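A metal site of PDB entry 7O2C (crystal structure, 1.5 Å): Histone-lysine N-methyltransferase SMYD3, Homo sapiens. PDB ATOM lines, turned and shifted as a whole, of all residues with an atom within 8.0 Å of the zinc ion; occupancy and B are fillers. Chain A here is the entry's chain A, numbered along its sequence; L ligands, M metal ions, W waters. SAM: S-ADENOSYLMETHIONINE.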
ATOM      1  N   HIS A 206      20.931   8.071 -13.770  1.00  0.00           N
ATOM      2  CA  HIS A 206      21.967   7.530 -12.840  1.00  0.00           C
ATOM      3  C   HIS A 206      23.330   8.136 -13.129  1.00  0.00           C
ATOM      4  O   HIS A 206      23.716   8.306 -14.275  1.00  0.00           O
ATOM      5  CB  HIS A 206      22.075   6.026 -13.013  1.00  0.00           C
ATOM      6  CG  HIS A 206      23.335   5.481 -12.435  1.00  0.00           C
ATOM      7  ND1 HIS A 206      23.383   5.166 -11.059  1.00  0.00           N
ATOM      8  CD2 HIS A 206      24.536   5.210 -12.951  1.00  0.00           C
ATOM      9  CE1 HIS A 206      24.632   4.760 -10.826  1.00  0.00           C
ATOM     10  NE2 HIS A 206      25.339   4.722 -11.980  1.00  0.00           N
ATOM     11  N   SER A 207      24.141   8.364 -12.095  1.00  0.00           N
ATOM     12  CA  SER A 207      25.577   8.641 -12.167  1.00  0.00           C
ATOM     13  C   SER A 207      26.218   7.892 -11.011  1.00  0.00           C
ATOM     14  O   SER A 207      25.644   7.832  -9.955  1.00  0.00           O
ATOM     15  CB  SER A 207      25.923  10.136 -12.097  1.00  0.00           C
ATOM     16  OG  SER A 207      27.322  10.292 -12.018  1.00  0.00           O
ATOM     17  N   CYS A 208      27.395   7.371 -11.253  1.00  0.00           N
ATOM     18  CA  CYS A 208      28.243   6.739 -10.246  1.00  0.00           C
ATOM     19  C   CYS A 208      28.935   7.845  -9.408  1.00  0.00           C
ATOM     20  O   CYS A 208      29.611   7.520  -8.400  1.00  0.00           O
ATOM     21  CB  CYS A 208      29.287   5.907 -10.936  1.00  0.00           C
ATOM     22  SG  CYS A 208      28.624   4.584 -11.957  1.00  0.00           S
ATOM     23  N   ASP A 209      28.762   9.113  -9.783  1.00  0.00           N
ATOM     24  CA  ASP A 209      29.289  10.265  -9.009  1.00  0.00           C
ATOM     25  C   ASP A 209      28.288  11.403  -9.170  1.00  0.00           C
ATOM     26  O   ASP A 209      28.538  12.349  -9.930  1.00  0.00           O
ATOM     27  CB  ASP A 209      30.681  10.656  -9.459  1.00  0.00           C
ATOM     28  CG  ASP A 209      31.237  11.862  -8.762  1.00  0.00           C
ATOM     29  OD1 ASP A 209      30.686  12.227  -7.702  1.00  0.00           O
ATOM     30  OD2 ASP A 209      32.204  12.343  -9.266  1.00  0.00           O
ATOM     31  N   LEU A 240      22.568   3.027  -7.093  1.00  0.00           N
ATOM     32  CA  LEU A 240      23.159   1.835  -6.426  1.00  0.00           C
ATOM     33  C   LEU A 240      23.811   2.182  -5.084  1.00  0.00           C
ATOM     34  O   LEU A 240      24.319   3.264  -4.870  1.00  0.00           O
ATOM     35  CB  LEU A 240      24.140   1.157  -7.363  1.00  0.00           C
ATOM     36  CG  LEU A 240      23.650   0.919  -8.788  1.00  0.00           C
ATOM     37  CD1 LEU A 240      24.858   0.386  -9.563  1.00  0.00           C
ATOM     38  CD2 LEU A 240      22.488  -0.099  -8.736  1.00  0.00           C
ATOM     39  N   SER A 246      33.098  -1.550  -9.975  1.00  0.00           N
ATOM     40  CA  SER A 246      32.656  -1.200 -11.339  1.00  0.00           C
ATOM     41  C   SER A 246      32.095  -2.467 -12.035  1.00  0.00           C
ATOM     42  O   SER A 246      31.086  -2.281 -12.742  1.00  0.00           O
ATOM     43  CB  SER A 246      33.742  -0.545 -12.151  1.00  0.00           C
ATOM     44  OG  SER A 246      34.818  -1.457 -12.413  1.00  0.00           O
ATOM     45  N   ARG A 249      28.619  -2.915 -10.484  1.00  0.00           N
ATOM     46  CA  ARG A 249      27.738  -1.868 -11.014  1.00  0.00           C
ATOM     47  C   ARG A 249      27.340  -2.218 -12.468  1.00  0.00           C
ATOM     48  O   ARG A 249      26.115  -2.111 -12.773  1.00  0.00           O
ATOM     49  CB  ARG A 249      28.384  -0.474 -10.937  1.00  0.00           C
ATOM     50  CG  ARG A 249      28.547   0.025  -9.509  1.00  0.00           C
ATOM     51  CD  ARG A 249      28.830   1.539  -9.443  1.00  0.00           C
ATOM     52  NE  ARG A 249      29.904   2.030 -10.291  1.00  0.00           N
ATOM     53  CZ  ARG A 249      31.216   2.055 -10.003  1.00  0.00           C
ATOM     54  NH1 ARG A 249      31.691   1.470  -8.896  1.00  0.00           N
ATOM     55  NH2 ARG A 249      32.078   2.473 -10.886  1.00  0.00           N
ATOM     56  N   ARG A 250      28.285  -2.689 -13.263  1.00  0.00           N
ATOM     57  CA  ARG A 250      27.990  -3.052 -14.664  1.00  0.00           C
ATOM     58  C   ARG A 250      26.902  -4.120 -14.703  1.00  0.00           C
ATOM     59  O   ARG A 250      25.927  -4.007 -15.500  1.00  0.00           O
ATOM     60  CB  ARG A 250      29.258  -3.558 -15.314  1.00  0.00           C
ATOM     61  CG  ARG A 250      29.017  -4.090 -16.731  1.00  0.00           C
ATOM     62  CD  ARG A 250      30.297  -4.403 -17.492  1.00  0.00           C
ATOM     63  NE  ARG A 250      31.029  -3.200 -17.757  1.00  0.00           N
ATOM     64  CZ  ARG A 250      32.151  -2.835 -17.128  1.00  0.00           C
ATOM     65  NH1 ARG A 250      32.754  -3.660 -16.293  1.00  0.00           N
ATOM     66  NH2 ARG A 250      32.686  -1.658 -17.404  1.00  0.00           N
ATOM     67  N   LEU A 253      23.470  -2.521 -13.505  1.00  0.00           N
ATOM     68  CA  LEU A 253      22.940  -1.527 -14.455  1.00  0.00           C
ATOM     69  C   LEU A 253      22.481  -2.213 -15.772  1.00  0.00           C
ATOM     70  O   LEU A 253      21.492  -1.731 -16.357  1.00  0.00           O
ATOM     71  CB  LEU A 253      23.938  -0.384 -14.692  1.00  0.00           C
ATOM     72  CG  LEU A 253      24.298   0.379 -13.408  1.00  0.00           C
ATOM     73  CD1 LEU A 253      25.402   1.340 -13.735  1.00  0.00           C
ATOM     74  CD2 LEU A 253      23.101   1.066 -12.865  1.00  0.00           C
ATOM     75  N   PHE A 259      21.363  -0.509 -19.291  1.00  0.00           N
ATOM     76  CA  PHE A 259      22.355   0.387 -19.879  1.00  0.00           C
ATOM     77  C   PHE A 259      23.771   0.137 -19.383  1.00  0.00           C
ATOM     78  O   PHE A 259      23.935  -0.618 -18.428  1.00  0.00           O
ATOM     79  CB  PHE A 259      22.003   1.865 -19.688  1.00  0.00           C
ATOM     80  CG  PHE A 259      22.242   2.417 -18.300  1.00  0.00           C
ATOM     81  CD1 PHE A 259      23.455   3.065 -17.996  1.00  0.00           C
ATOM     82  CD2 PHE A 259      21.261   2.301 -17.331  1.00  0.00           C
ATOM     83  CE1 PHE A 259      23.633   3.523 -16.685  1.00  0.00           C
ATOM     84  CE2 PHE A 259      21.464   2.726 -16.030  1.00  0.00           C
ATOM     85  CZ  PHE A 259      22.628   3.402 -15.739  1.00  0.00           C
ATOM     86  N   GLU A 260      24.685   0.618 -20.208  1.00  0.00           N
ATOM     87  CA  GLU A 260      26.150   0.526 -20.087  1.00  0.00           C
ATOM     88  C   GLU A 260      26.608   1.893 -19.603  1.00  0.00           C
ATOM     89  O   GLU A 260      26.314   2.921 -20.195  1.00  0.00           O
ATOM     90  CB  GLU A 260      26.762   0.240 -21.465  1.00  0.00           C
ATOM     91  CG  GLU A 260      26.079  -0.912 -22.243  1.00  0.00           C
ATOM     92  CD  GLU A 260      26.035  -2.262 -21.578  1.00  0.00           C
ATOM     93  OE1 GLU A 260      26.778  -2.534 -20.560  1.00  0.00           O
ATOM     94  OE2 GLU A 260      25.243  -3.137 -22.062  1.00  0.00           O
ATOM     95  N   CYS A 261      27.422   1.914 -18.551  1.00  0.00           N
ATOM     96  CA  CYS A 261      27.938   3.209 -18.076  1.00  0.00           C
ATOM     97  C   CYS A 261      29.382   3.436 -18.498  1.00  0.00           C
ATOM     98  O   CYS A 261      30.225   2.567 -18.236  1.00  0.00           O
ATOM     99  CB  CYS A 261      27.806   3.272 -16.561  1.00  0.00           C
ATOM    100  SG  CYS A 261      28.346   4.887 -15.895  1.00  0.00           S
ATOM    101  N   ASP A 262      29.634   4.556 -19.187  1.00  0.00           N
ATOM    102  CA  ASP A 262      31.032   4.886 -19.594  1.00  0.00           C
ATOM    103  C   ASP A 262      31.508   6.133 -18.845  1.00  0.00           C
ATOM    104  O   ASP A 262      32.441   6.771 -19.439  1.00  0.00           O
ATOM    105  CB  ASP A 262      31.216   4.945 -21.130  1.00  0.00           C
ATOM    106  CG  ASP A 262      30.646   6.188 -21.779  1.00  0.00           C
ATOM    107  OD1 ASP A 262      29.678   6.766 -21.141  1.00  0.00           O
ATOM    108  OD2 ASP A 262      31.138   6.538 -22.931  1.00  0.00           O
ATOM    109  N   CYS A 263      31.029   6.353 -17.601  1.00  0.00           N
ATOM    110  CA  CYS A 263      31.522   7.478 -16.780  1.00  0.00           C
ATOM    111  C   CYS A 263      32.977   7.267 -16.439  1.00  0.00           C
ATOM    112  O   CYS A 263      33.518   6.164 -16.607  1.00  0.00           O
ATOM    113  CB  CYS A 263      30.717   7.670 -15.506  1.00  0.00           C
ATOM    114  SG  CYS A 263      31.097   6.559 -14.120  1.00  0.00           S
ATOM    115  N   PHE A 264      33.577   8.334 -15.937  1.00  0.00           N
ATOM    116  CA  PHE A 264      34.990   8.291 -15.562  1.00  0.00           C
ATOM    117  C   PHE A 264      35.251   7.139 -14.581  1.00  0.00           C
ATOM    118  O   PHE A 264      36.286   6.470 -14.676  1.00  0.00           O
ATOM    119  CB  PHE A 264      35.371   9.629 -14.934  1.00  0.00           C
ATOM    120  CG  PHE A 264      36.727   9.574 -14.280  1.00  0.00           C
ATOM    121  CD1 PHE A 264      37.893   9.524 -15.023  1.00  0.00           C
ATOM    122  CD2 PHE A 264      36.812   9.494 -12.892  1.00  0.00           C
ATOM    123  CE1 PHE A 264      39.133   9.417 -14.417  1.00  0.00           C
ATOM    124  CE2 PHE A 264      38.060   9.391 -12.290  1.00  0.00           C
ATOM    125  CZ  PHE A 264      39.211   9.363 -13.059  1.00  0.00           C
ATOM    126  N   ARG A 265      34.395   6.998 -13.574  1.00  0.00           N
ATOM    127  CA  ARG A 265      34.612   5.967 -12.539  1.00  0.00           C
ATOM    128  C   ARG A 265      34.603   4.575 -13.128  1.00  0.00           C
ATOM    129  O   ARG A 265      35.490   3.786 -12.811  1.00  0.00           O
ATOM    130  CB  ARG A 265      33.602   6.032 -11.397  1.00  0.00           C
ATOM    131  CG  ARG A 265      33.671   7.294 -10.545  1.00  0.00           C
ATOM    132  CD  ARG A 265      32.886   7.182  -9.269  1.00  0.00           C
ATOM    133  NE  ARG A 265      33.476   6.152  -8.422  1.00  0.00           N
ATOM    134  CZ  ARG A 265      32.853   5.180  -7.774  1.00  0.00           C
ATOM    135  NH1 ARG A 265      31.525   5.133  -7.682  1.00  0.00           N
ATOM    136  NH2 ARG A 265      33.571   4.222  -7.245  1.00  0.00           N
ATOM    137  N   CYS A 266      33.670   4.323 -14.047  1.00  0.00           N
ATOM    138  CA  CYS A 266      33.592   2.966 -14.678  1.00  0.00           C
ATOM    139  C   CYS A 266      34.753   2.752 -15.678  1.00  0.00           C
ATOM    140  O   CYS A 266      35.331   1.640 -15.708  1.00  0.00           O
ATOM    141  CB  CYS A 266      32.204   2.734 -15.315  1.00  0.00           C
ATOM    142  SG  CYS A 266      30.906   2.677 -14.056  1.00  0.00           S
ATOM    143  N   GLN A 267      35.103   3.782 -16.430  1.00  0.00           N
ATOM    144  CA  GLN A 267      36.272   3.698 -17.367  1.00  0.00           C
ATOM    145  C   GLN A 267      37.595   3.433 -16.634  1.00  0.00           C
ATOM    146  O   GLN A 267      38.537   2.826 -17.193  1.00  0.00           O
ATOM    147  CB  GLN A 267      36.378   4.959 -18.197  1.00  0.00           C
ATOM    148  CG  GLN A 267      35.347   4.967 -19.286  1.00  0.00           C
ATOM    149  CD  GLN A 267      35.852   5.631 -20.525  1.00  0.00           C
ATOM    150  OE1 GLN A 267      37.023   5.467 -20.977  1.00  0.00           O
ATOM    151  NE2 GLN A 267      34.967   6.470 -21.010  1.00  0.00           N
HETATM  152  N   SAM L   1      15.742   8.024 -18.815  1.00  0.00           N
HETATM  153  CA  SAM L   1      14.527   7.588 -18.066  1.00  0.00           C
HETATM  154  C   SAM L   1      13.235   7.949 -18.836  1.00  0.00           C
HETATM  155  O   SAM L   1      12.186   7.800 -18.284  1.00  0.00           O
HETATM  156  OXT SAM L   1      13.400   8.285 -20.033  1.00  0.00           O
HETATM  157  CB  SAM L   1      14.513   8.191 -16.651  1.00  0.00           C
HETATM  158  CG  SAM L   1      15.333   7.352 -15.659  1.00  0.00           C
HETATM  159  SD  SAM L   1      14.540   5.781 -15.325  1.00  0.00           S
HETATM  160  CE  SAM L   1      14.440   5.647 -13.568  1.00  0.00           C
HETATM  161  C5' SAM L   1      15.853   4.569 -15.561  1.00  0.00           C
HETATM  162  C4' SAM L   1      16.275   4.301 -17.005  1.00  0.00           C
HETATM  163  O4' SAM L   1      16.863   5.486 -17.569  1.00  0.00           O
HETATM  164  C3' SAM L   1      17.305   3.215 -17.218  1.00  0.00           C
HETATM  165  O3' SAM L   1      16.709   1.930 -17.139  1.00  0.00           O
HETATM  166  C2' SAM L   1      17.913   3.621 -18.576  1.00  0.00           C
HETATM  167  O2' SAM L   1      16.980   3.354 -19.614  1.00  0.00           O
HETATM  168  C1' SAM L   1      17.954   5.144 -18.413  1.00  0.00           C
HETATM  169  N9  SAM L   1      19.190   5.622 -17.793  1.00  0.00           N
HETATM  170  C8  SAM L   1      19.383   6.064 -16.494  1.00  0.00           C
HETATM  171  N7  SAM L   1      20.620   6.449 -16.251  1.00  0.00           N
HETATM  172  C5  SAM L   1      21.299   6.263 -17.430  1.00  0.00           C
HETATM  173  C6  SAM L   1      22.631   6.490 -17.784  1.00  0.00           C
HETATM  174  N6  SAM L   1      23.533   7.051 -16.967  1.00  0.00           N
HETATM  175  N1  SAM L   1      23.027   6.172 -19.039  1.00  0.00           N
HETATM  176  C2  SAM L   1      22.081   5.643 -19.861  1.00  0.00           C
HETATM  177  N3  SAM L   1      20.789   5.412 -19.636  1.00  0.00           N
HETATM  178  C4  SAM L   1      20.423   5.749 -18.378  1.00  0.00           C
HETATM  179 ZN    ZN M   1      29.653   4.668 -14.064  1.00  0.00          ZN
HETATM  180  O   HOH W   1      27.861   7.590 -14.367  1.00  0.00           O
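The zinc ion is bound by SG of Cys 261. SG of Cys 208 binds the zinc ion (2.3 Å). The side-chain sulfur (SG) of Cys 266 is bound to the zinc ion (2.4 Å). The zinc ion is bound by the side-chain sulfur (SG) of Cys 263 (2.4 Å).
NE of Arg 249 sits close to SG of Cys 208 (3.3 Å). The backbone NH (N) of Cys 208 is in hydrogen-bond range of a ring nitrogen (NE2) of His 206 (3.4 Å). O of Cys 208 lies within hydrogen-bond range of NH1 of Arg 265 (3.1 Å). The guanidinium group of Arg 249 sits close to the side-chain sulfur of Cys 266, 3.4 Å away. SG of Cys 263 sits close to N of Arg 265, at 3.4 Å.
N7 of the ligand sits at hydrogen-bond distance from N of His 206 (3.0 Å). A nitrogen (N6) of the ligand sits at hydrogen-bond distance from the backbone carbonyl oxygen (O) of His 206, at 3.0 Å.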
